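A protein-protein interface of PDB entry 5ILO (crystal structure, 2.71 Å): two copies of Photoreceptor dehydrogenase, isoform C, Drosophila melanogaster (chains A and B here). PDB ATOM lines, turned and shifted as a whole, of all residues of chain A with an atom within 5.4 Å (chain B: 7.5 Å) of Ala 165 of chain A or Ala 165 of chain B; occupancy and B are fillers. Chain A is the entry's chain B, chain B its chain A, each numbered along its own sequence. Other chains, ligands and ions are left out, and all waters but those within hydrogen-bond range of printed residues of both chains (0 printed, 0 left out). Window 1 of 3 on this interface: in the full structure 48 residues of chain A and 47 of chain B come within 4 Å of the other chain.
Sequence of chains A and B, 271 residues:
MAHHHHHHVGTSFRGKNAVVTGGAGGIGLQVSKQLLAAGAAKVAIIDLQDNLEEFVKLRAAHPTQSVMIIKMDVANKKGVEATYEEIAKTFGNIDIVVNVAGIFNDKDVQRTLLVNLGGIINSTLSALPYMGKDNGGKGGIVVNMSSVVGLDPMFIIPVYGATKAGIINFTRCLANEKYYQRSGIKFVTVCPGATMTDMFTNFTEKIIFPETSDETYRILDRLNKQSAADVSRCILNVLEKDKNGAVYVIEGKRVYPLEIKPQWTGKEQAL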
ATOM      1  N   SER A 146     -23.113   3.197 -10.147  1.00  0.00           N
ATOM      2  CA  SER A 146     -23.271   3.842  -8.852  1.00  0.00           C
ATOM      3  C   SER A 146     -22.843   5.300  -8.966  1.00  0.00           C
ATOM      4  O   SER A 146     -22.935   5.894 -10.040  1.00  0.00           O
ATOM      5  CB  SER A 146     -22.455   3.114  -7.783  1.00  0.00           C
ATOM      6  OG  SER A 146     -22.641   3.703  -6.508  1.00  0.00           O
ATOM      7  N   GLY A 150     -21.909   7.706  -3.532  1.00  0.00           N
ATOM      8  CA  GLY A 150     -22.100   6.395  -2.937  1.00  0.00           C
ATOM      9  C   GLY A 150     -20.944   6.004  -2.037  1.00  0.00           C
ATOM     10  O   GLY A 150     -21.132   5.328  -1.027  1.00  0.00           O
ATOM     11  N   GLY A 161     -27.890   9.486  -2.573  1.00  0.00           N
ATOM     12  CA  GLY A 161     -26.638   8.932  -2.090  1.00  0.00           C
ATOM     13  C   GLY A 161     -26.788   7.556  -1.469  1.00  0.00           C
ATOM     14  O   GLY A 161     -26.049   6.630  -1.811  1.00  0.00           O
ATOM     15  N   ALA A 162     -27.740   7.430  -0.547  1.00  0.00           N
ATOM     16  CA  ALA A 162     -28.046   6.159   0.107  1.00  0.00           C
ATOM     17  C   ALA A 162     -28.196   4.997  -0.874  1.00  0.00           C
ATOM     18  O   ALA A 162     -27.672   3.909  -0.638  1.00  0.00           O
ATOM     19  CB  ALA A 162     -29.312   6.297   0.942  1.00  0.00           C
ATOM     20  N   THR A 163     -28.913   5.229  -1.972  1.00  0.00           N
ATOM     21  CA  THR A 163     -29.160   4.176  -2.958  1.00  0.00           C
ATOM     22  C   THR A 163     -27.872   3.765  -3.654  1.00  0.00           C
ATOM     23  O   THR A 163     -27.729   2.626  -4.083  1.00  0.00           O
ATOM     24  CB  THR A 163     -30.183   4.601  -4.036  1.00  0.00           C
ATOM     25  OG1 THR A 163     -29.703   5.755  -4.736  1.00  0.00           O
ATOM     26  CG2 THR A 163     -31.532   4.904  -3.407  1.00  0.00           C
ATOM     27  N   LYS A 164     -26.945   4.708  -3.770  1.00  0.00           N
ATOM     28  CA  LYS A 164     -25.675   4.465  -4.440  1.00  0.00           C
ATOM     29  C   LYS A 164     -24.713   3.695  -3.539  1.00  0.00           C
ATOM     30  O   LYS A 164     -23.962   2.837  -4.004  1.00  0.00           O
ATOM     31  CB  LYS A 164     -25.056   5.789  -4.892  1.00  0.00           C
ATOM     32  CG  LYS A 164     -25.922   6.532  -5.892  1.00  0.00           C
ATOM     33  CD  LYS A 164     -25.935   5.816  -7.227  1.00  0.00           C
ATOM     34  CE  LYS A 164     -27.172   6.171  -8.025  1.00  0.00           C
ATOM     35  NZ  LYS A 164     -27.281   5.350  -9.263  1.00  0.00           N
ATOM     36  N   ALA A 165     -24.735   4.019  -2.250  1.00  0.00           N
ATOM     37  CA  ALA A 165     -24.019   3.242  -1.246  1.00  0.00           C
ATOM     38  C   ALA A 165     -24.543   1.811  -1.207  1.00  0.00           C
ATOM     39  O   ALA A 165     -23.783   0.860  -1.017  1.00  0.00           O
ATOM     40  CB  ALA A 165     -24.147   3.893   0.115  1.00  0.00           C
ATOM     41  N   GLY A 166     -25.856   1.675  -1.363  1.00  0.00           N
ATOM     42  CA  GLY A 166     -26.500   0.377  -1.399  1.00  0.00           C
ATOM     43  C   GLY A 166     -26.086  -0.443  -2.605  1.00  0.00           C
ATOM     44  O   GLY A 166     -25.879  -1.652  -2.503  1.00  0.00           O
ATOM     45  N   ILE A 167     -25.967   0.221  -3.752  1.00  0.00           N
ATOM     46  CA  ILE A 167     -25.567  -0.434  -4.993  1.00  0.00           C
ATOM     47  C   ILE A 167     -24.169  -1.028  -4.853  1.00  0.00           C
ATOM     48  O   ILE A 167     -23.946  -2.192  -5.188  1.00  0.00           O
ATOM     49  CB  ILE A 167     -25.612   0.540  -6.188  1.00  0.00           C
ATOM     50  CG1 ILE A 167     -27.066   0.806  -6.591  1.00  0.00           C
ATOM     51  CG2 ILE A 167     -24.843  -0.024  -7.373  1.00  0.00           C
ATOM     52  CD1 ILE A 167     -27.259   2.048  -7.426  1.00  0.00           C
ATOM     53  N   ILE A 168     -23.236  -0.219  -4.357  1.00  0.00           N
ATOM     54  CA  ILE A 168     -21.859  -0.652  -4.153  1.00  0.00           C
ATOM     55  C   ILE A 168     -21.805  -1.896  -3.274  1.00  0.00           C
ATOM     56  O   ILE A 168     -21.242  -2.919  -3.670  1.00  0.00           O
ATOM     57  CB  ILE A 168     -21.006   0.454  -3.507  1.00  0.00           C
ATOM     58  CG1 ILE A 168     -20.919   1.670  -4.430  1.00  0.00           C
ATOM     59  CG2 ILE A 168     -19.618  -0.068  -3.172  1.00  0.00           C
ATOM     60  CD1 ILE A 168     -20.473   2.936  -3.732  1.00  0.00           C
ATOM     61  N   ASN A 169     -22.393  -1.795  -2.084  1.00  0.00           N
ATOM     62  CA  ASN A 169     -22.384  -2.882  -1.112  1.00  0.00           C
ATOM     63  C   ASN A 169     -23.049  -4.145  -1.661  1.00  0.00           C
ATOM     64  O   ASN A 169     -22.544  -5.252  -1.477  1.00  0.00           O
ATOM     65  CB  ASN A 169     -23.072  -2.424   0.177  1.00  0.00           C
ATOM     66  CG  ASN A 169     -23.179  -3.525   1.223  1.00  0.00           C
ATOM     67  OD1 ASN A 169     -23.917  -4.497   1.054  1.00  0.00           O
ATOM     68  ND2 ASN A 169     -22.450  -3.365   2.320  1.00  0.00           N
ATOM     69  N   PHE A 170     -24.186  -3.970  -2.330  1.00  0.00           N
ATOM     70  CA  PHE A 170     -24.870  -5.072  -3.002  1.00  0.00           C
ATOM     71  C   PHE A 170     -23.970  -5.788  -4.015  1.00  0.00           C
ATOM     72  O   PHE A 170     -23.821  -7.012  -3.970  1.00  0.00           O
ATOM     73  CB  PHE A 170     -26.133  -4.565  -3.703  1.00  0.00           C
ATOM     74  CG  PHE A 170     -26.836  -5.613  -4.513  1.00  0.00           C
ATOM     75  CD1 PHE A 170     -27.571  -6.608  -3.894  1.00  0.00           C
ATOM     76  CD2 PHE A 170     -26.742  -5.613  -5.899  1.00  0.00           C
ATOM     77  CE1 PHE A 170     -28.214  -7.578  -4.643  1.00  0.00           C
ATOM     78  CE2 PHE A 170     -27.381  -6.578  -6.655  1.00  0.00           C
ATOM     79  CZ  PHE A 170     -28.118  -7.563  -6.026  1.00  0.00           C
ATOM     80  N   LEU B 117     -34.484   0.709   4.619  1.00  0.00           N
ATOM     81  CA  LEU B 117     -33.938   2.005   4.233  1.00  0.00           C
ATOM     82  C   LEU B 117     -35.002   3.103   4.241  1.00  0.00           C
ATOM     83  O   LEU B 117     -34.792   4.177   4.805  1.00  0.00           O
ATOM     84  CB  LEU B 117     -33.286   1.916   2.851  1.00  0.00           C
ATOM     85  CG  LEU B 117     -32.581   3.175   2.341  1.00  0.00           C
ATOM     86  CD1 LEU B 117     -31.548   3.661   3.343  1.00  0.00           C
ATOM     87  CD2 LEU B 117     -31.931   2.889   0.998  1.00  0.00           C
ATOM     88  N   SER B 146     -28.200   0.465  11.895  1.00  0.00           N
ATOM     89  CA  SER B 146     -27.624  -0.143  10.706  1.00  0.00           C
ATOM     90  C   SER B 146     -27.058  -1.508  11.073  1.00  0.00           C
ATOM     91  O   SER B 146     -27.506  -2.128  12.036  1.00  0.00           O
ATOM     92  CB  SER B 146     -26.537   0.751  10.113  1.00  0.00           C
ATOM     93  OG  SER B 146     -26.003   0.187   8.928  1.00  0.00           O
ATOM     94  N   SER B 147     -26.101  -1.988  10.289  1.00  0.00           N
ATOM     95  CA  SER B 147     -25.452  -3.259  10.583  1.00  0.00           C
ATOM     96  C   SER B 147     -23.953  -3.182  10.322  1.00  0.00           C
ATOM     97  O   SER B 147     -23.474  -2.252   9.667  1.00  0.00           O
ATOM     98  CB  SER B 147     -26.067  -4.379   9.752  1.00  0.00           C
ATOM     99  OG  SER B 147     -25.324  -5.577   9.897  1.00  0.00           O
ATOM    100  N   VAL B 149     -22.652  -5.433   8.429  1.00  0.00           N
ATOM    101  CA  VAL B 149     -22.640  -5.805   7.020  1.00  0.00           C
ATOM    102  C   VAL B 149     -22.887  -4.580   6.142  1.00  0.00           C
ATOM    103  O   VAL B 149     -22.596  -4.595   4.941  1.00  0.00           O
ATOM    104  CB  VAL B 149     -23.692  -6.886   6.699  1.00  0.00           C
ATOM    105  CG1 VAL B 149     -23.557  -8.054   7.660  1.00  0.00           C
ATOM    106  CG2 VAL B 149     -25.096  -6.315   6.769  1.00  0.00           C
ATOM    107  N   GLY B 150     -23.440  -3.528   6.744  1.00  0.00           N
ATOM    108  CA  GLY B 150     -23.561  -2.244   6.078  1.00  0.00           C
ATOM    109  C   GLY B 150     -22.204  -1.640   5.782  1.00  0.00           C
ATOM    110  O   GLY B 150     -22.020  -0.971   4.765  1.00  0.00           O
ATOM    111  N   LEU B 151     -21.250  -1.889   6.674  1.00  0.00           N
ATOM    112  CA  LEU B 151     -19.885  -1.405   6.504  1.00  0.00           C
ATOM    113  C   LEU B 151     -19.086  -2.357   5.629  1.00  0.00           C
ATOM    114  O   LEU B 151     -18.460  -1.945   4.649  1.00  0.00           O
ATOM    115  CB  LEU B 151     -19.196  -1.254   7.861  1.00  0.00           C
ATOM    116  CG  LEU B 151     -19.848  -0.317   8.878  1.00  0.00           C
ATOM    117  CD1 LEU B 151     -19.517  -0.762  10.294  1.00  0.00           C
ATOM    118  CD2 LEU B 151     -19.404   1.120   8.645  1.00  0.00           C
ATOM    119  N   ASP B 152     -19.128  -3.635   5.986  1.00  0.00           N
ATOM    120  CA  ASP B 152     -18.400  -4.662   5.259  1.00  0.00           C
ATOM    121  C   ASP B 152     -19.385  -5.686   4.723  1.00  0.00           C
ATOM    122  O   ASP B 152     -19.972  -6.441   5.494  1.00  0.00           O
ATOM    123  CB  ASP B 152     -17.366  -5.339   6.163  1.00  0.00           C
ATOM    124  CG  ASP B 152     -16.360  -4.360   6.741  1.00  0.00           C
ATOM    125  OD1 ASP B 152     -16.229  -3.240   6.201  1.00  0.00           O
ATOM    126  OD2 ASP B 152     -15.703  -4.706   7.744  1.00  0.00           O
ATOM    127  N   PRO B 153     -19.562  -5.719   3.393  1.00  0.00           N
ATOM    128  CA  PRO B 153     -20.579  -6.555   2.741  1.00  0.00           C
ATOM    129  C   PRO B 153     -20.517  -8.018   3.166  1.00  0.00           C
ATOM    130  O   PRO B 153     -19.427  -8.578   3.296  1.00  0.00           O
ATOM    131  CB  PRO B 153     -20.245  -6.421   1.252  1.00  0.00           C
ATOM    132  CG  PRO B 153     -19.520  -5.134   1.136  1.00  0.00           C
ATOM    133  CD  PRO B 153     -18.786  -4.925   2.425  1.00  0.00           C
ATOM    134  N   VAL B 159     -29.069  -8.102  -0.304  1.00  0.00           N
ATOM    135  CA  VAL B 159     -30.144  -7.107  -0.325  1.00  0.00           C
ATOM    136  C   VAL B 159     -30.247  -6.386   1.013  1.00  0.00           C
ATOM    137  O   VAL B 159     -30.263  -5.154   1.072  1.00  0.00           O
ATOM    138  CB  VAL B 159     -31.506  -7.742  -0.656  1.00  0.00           C
ATOM    139  CG1 VAL B 159     -32.600  -6.683  -0.658  1.00  0.00           C
ATOM    140  CG2 VAL B 159     -31.447  -8.456  -1.997  1.00  0.00           C
ATOM    141  N   TYR B 160     -30.343  -7.172   2.079  1.00  0.00           N
ATOM    142  CA  TYR B 160     -30.383  -6.655   3.439  1.00  0.00           C
ATOM    143  C   TYR B 160     -29.176  -5.756   3.708  1.00  0.00           C
ATOM    144  O   TYR B 160     -29.301  -4.703   4.331  1.00  0.00           O
ATOM    145  CB  TYR B 160     -30.443  -7.819   4.435  1.00  0.00           C
ATOM    146  CG  TYR B 160     -30.208  -7.439   5.880  1.00  0.00           C
ATOM    147  CD1 TYR B 160     -28.925  -7.424   6.418  1.00  0.00           C
ATOM    148  CD2 TYR B 160     -31.270  -7.091   6.706  1.00  0.00           C
ATOM    149  CE1 TYR B 160     -28.710  -7.074   7.734  1.00  0.00           C
ATOM    150  CE2 TYR B 160     -31.064  -6.742   8.025  1.00  0.00           C
ATOM    151  CZ  TYR B 160     -29.783  -6.734   8.532  1.00  0.00           C
ATOM    152  OH  TYR B 160     -29.577  -6.386   9.843  1.00  0.00           O
ATOM    153  N   GLY B 161     -28.010  -6.197   3.246  1.00  0.00           N
ATOM    154  CA  GLY B 161     -26.775  -5.440   3.366  1.00  0.00           C
ATOM    155  C   GLY B 161     -26.826  -4.084   2.687  1.00  0.00           C
ATOM    156  O   GLY B 161     -26.461  -3.069   3.281  1.00  0.00           O
ATOM    157  N   ALA B 162     -27.257  -4.080   1.428  1.00  0.00           N
ATOM    158  CA  ALA B 162     -27.422  -2.853   0.652  1.00  0.00           C
ATOM    159  C   ALA B 162     -28.183  -1.766   1.412  1.00  0.00           C
ATOM    160  O   ALA B 162     -27.783  -0.600   1.400  1.00  0.00           O
ATOM    161  CB  ALA B 162     -28.127  -3.160  -0.661  1.00  0.00           C
ATOM    162  N   THR B 163     -29.275  -2.147   2.071  1.00  0.00           N
ATOM    163  CA  THR B 163     -30.111  -1.182   2.789  1.00  0.00           C
ATOM    164  C   THR B 163     -29.371  -0.591   3.978  1.00  0.00           C
ATOM    165  O   THR B 163     -29.609   0.553   4.362  1.00  0.00           O
ATOM    166  CB  THR B 163     -31.430  -1.806   3.302  1.00  0.00           C
ATOM    167  OG1 THR B 163     -31.141  -2.892   4.193  1.00  0.00           O
ATOM    168  CG2 THR B 163     -32.274  -2.303   2.145  1.00  0.00           C
ATOM    169  N   LYS B 164     -28.471  -1.378   4.553  1.00  0.00           N
ATOM    170  CA  LYS B 164     -27.709  -0.958   5.719  1.00  0.00           C
ATOM    171  C   LYS B 164     -26.584  -0.005   5.322  1.00  0.00           C
ATOM    172  O   LYS B 164     -26.301   0.967   6.024  1.00  0.00           O
ATOM    173  CB  LYS B 164     -27.156  -2.183   6.450  1.00  0.00           C
ATOM    174  CG  LYS B 164     -28.241  -3.107   6.981  1.00  0.00           C
ATOM    175  CD  LYS B 164     -28.960  -2.473   8.161  1.00  0.00           C
ATOM    176  CE  LYS B 164     -30.344  -3.057   8.355  1.00  0.00           C
ATOM    177  NZ  LYS B 164     -31.091  -2.322   9.412  1.00  0.00           N
ATOM    178  N   ALA B 165     -25.951  -0.288   4.189  1.00  0.00           N
ATOM    179  CA  ALA B 165     -24.985   0.629   3.595  1.00  0.00           C
ATOM    180  C   ALA B 165     -25.660   1.949   3.252  1.00  0.00           C
ATOM    181  O   ALA B 165     -25.071   3.019   3.396  1.00  0.00           O
ATOM    182  CB  ALA B 165     -24.356   0.017   2.364  1.00  0.00           C
ATOM    183  N   GLY B 166     -26.898   1.855   2.781  1.00  0.00           N
ATOM    184  CA  GLY B 166     -27.695   3.022   2.458  1.00  0.00           C
ATOM    185  C   GLY B 166     -28.009   3.856   3.684  1.00  0.00           C
ATOM    186  O   GLY B 166     -27.996   5.084   3.629  1.00  0.00           O
ATOM    187  N   ILE B 167     -28.304   3.183   4.794  1.00  0.00           N
ATOM    188  CA  ILE B 167     -28.612   3.860   6.051  1.00  0.00           C
ATOM    189  C   ILE B 167     -27.413   4.680   6.529  1.00  0.00           C
ATOM    190  O   ILE B 167     -27.555   5.856   6.863  1.00  0.00           O
ATOM    191  CB  ILE B 167     -29.040   2.854   7.143  1.00  0.00           C
ATOM    192  CG1 ILE B 167     -30.455   2.341   6.862  1.00  0.00           C
ATOM    193  CG2 ILE B 167     -28.989   3.496   8.520  1.00  0.00           C
ATOM    194  CD1 ILE B 167     -30.799   1.055   7.578  1.00  0.00           C
ATOM    195  N   ILE B 168     -26.238   4.053   6.551  1.00  0.00           N
ATOM    196  CA  ILE B 168     -25.002   4.709   6.977  1.00  0.00           C
ATOM    197  C   ILE B 168     -24.747   5.976   6.171  1.00  0.00           C
ATOM    198  O   ILE B 168     -24.580   7.057   6.739  1.00  0.00           O
ATOM    199  CB  ILE B 168     -23.781   3.778   6.840  1.00  0.00           C
ATOM    200  CG1 ILE B 168     -23.920   2.575   7.774  1.00  0.00           C
ATOM    201  CG2 ILE B 168     -22.493   4.531   7.143  1.00  0.00           C
ATOM    202  CD1 ILE B 168     -23.006   1.416   7.428  1.00  0.00           C
ATOM    203  N   ASN B 169     -24.707   5.831   4.850  1.00  0.00           N
ATOM    204  CA  ASN B 169     -24.431   6.950   3.957  1.00  0.00           C
ATOM    205  C   ASN B 169     -25.465   8.069   4.108  1.00  0.00           C
ATOM    206  O   ASN B 169     -25.109   9.248   4.150  1.00  0.00           O
ATOM    207  CB  ASN B 169     -24.379   6.453   2.510  1.00  0.00           C
ATOM    208  CG  ASN B 169     -24.173   7.573   1.496  1.00  0.00           C
ATOM    209  OD1 ASN B 169     -25.051   8.409   1.278  1.00  0.00           O
ATOM    210  ND2 ASN B 169     -23.006   7.583   0.863  1.00  0.00           N
ATOM    211  N   PHE B 170     -26.738   7.692   4.192  1.00  0.00           N
ATOM    212  CA  PHE B 170     -27.822   8.644   4.434  1.00  0.00           C
ATOM    213  C   PHE B 170     -27.600   9.457   5.711  1.00  0.00           C
ATOM    214  O   PHE B 170     -27.649  10.687   5.694  1.00  0.00           O
ATOM    215  CB  PHE B 170     -29.165   7.907   4.508  1.00  0.00           C
ATOM    216  CG  PHE B 170     -30.324   8.791   4.864  1.00  0.00           C
ATOM    217  CD1 PHE B 170     -30.848   9.676   3.939  1.00  0.00           C
ATOM    218  CD2 PHE B 170     -30.886   8.742   6.133  1.00  0.00           C
ATOM    219  CE1 PHE B 170     -31.915  10.495   4.268  1.00  0.00           C
ATOM    220  CE2 PHE B 170     -31.951   9.558   6.471  1.00  0.00           C
ATOM    221  CZ  PHE B 170     -32.468  10.436   5.537  1.00  0.00           C
ATOM    222  N   THR B 171     -27.372   8.755   6.816  1.00  0.00           N
ATOM    223  CA  THR B 171     -27.244   9.380   8.130  1.00  0.00           C
ATOM    224  C   THR B 171     -26.032  10.312   8.212  1.00  0.00           C
ATOM    225  O   THR B 171     -26.084  11.362   8.859  1.00  0.00           O
ATOM    226  CB  THR B 171     -27.137   8.314   9.244  1.00  0.00           C
ATOM    227  OG1 THR B 171     -28.197   7.361   9.104  1.00  0.00           O
ATOM    228  CG2 THR B 171     -27.201   8.957  10.623  1.00  0.00           C
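The side-chain amide oxygen of Asn 169 of chain B sits at hydrogen-bond distance from the backbone NH of Ala 162 of chain A (3.4 Å). The side-chain amide nitrogen (ND2) of Asn 169 of chain A sits at hydrogen-bond distance from the backbone carbonyl oxygen (O) of Gly 150 of chain B. OD1 of Asn 169 of chain A sits at hydrogen-bond distance from N of Ala 162 of chain B. The side-chain amide nitrogen (ND2) of Asn 169 of chain B lies within hydrogen-bond range of the backbone carbonyl oxygen (O) of Gly 150 of chain A. The backbone carbonyl oxygen (O) of Val 149 of chain B lies within hydrogen-bond range of the side-chain amide nitrogen (ND2) of Asn 169 of chain A, 2.9 Å away.
OG of Ser 147 of chain B is in hydrogen-bond range of N of Val 149 of chain B (3.1 Å).
Among the printed residues, merely in contact across the chains: Ala 162 of chain A with Gly 166 of chain B, Gly 166 of chain A with Ala 162 of chain B, Gly 161 of chain A with Asn 169 of chain B, Asn 169 of chain A with Gly 161 of chain B, Ala 165 of chain A with Asn 169 of chain B, Ala 165 of chain A with Ala 165 of chain B, Asn 169 of chain A with Ala 165 of chain B, Asn 169 of chain A with Pro 153 of chain B, Phe 170 of chain A with Ala 162 of chain B and Ala 162 of chain A with Phe 170 of chain B.
Ala 165 of chain A touches two residues of chain B. Ala 165 of chain B touches just these residues of chain A: Ala 165 and Asn 169. Of the printed residues of chain A, Pro 153 of chain B touches Asn 169. Of the printed residues of chain B, Gly 150 of chain A touches Asn 169 (3.5 Å). Tyr 160 of chain B touches none of the printed residues of chain A. Ser 147 of chain B touches none of the printed residues of chain A. The nearest residue of chain A that does not touch Ala 165 of chain B is Gly 166 of chain A (4.3 Å).
Of the 21 printed residues of chain B, 9 touch a printed residue of chain A. Hydrophobic or aromatic side chains of chain B that line the printed part of chain A: Pro 153, Ala 162, Ala 165 and Phe 170. Hydrophobic or aromatic side chains of chain A that line the printed part of chain B: Ala 162, Ala 165 and Phe 170. Among the printed residues, no Asp or Glu carboxylate lies within 4 Å of a Lys or Arg side-chain nitrogen of the other chain.
Ala 162 of chain A touches Asn 169 of chain B, and with the chains exchanged Asn 169 of chain A touches Ala 162 of chain B. Ala 162 of chain A touches Phe 170 of chain B, and with the chains exchanged Phe 170 of chain A touches Ala 162 of chain B. Ala 165 of chain A touches its own counterpart, Ala 165 of chain B. Ala 165 of chain A touches Asn 169 of chain B, and with the chains exchanged Asn 169 of chain A touches Ala 165 of chain B.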
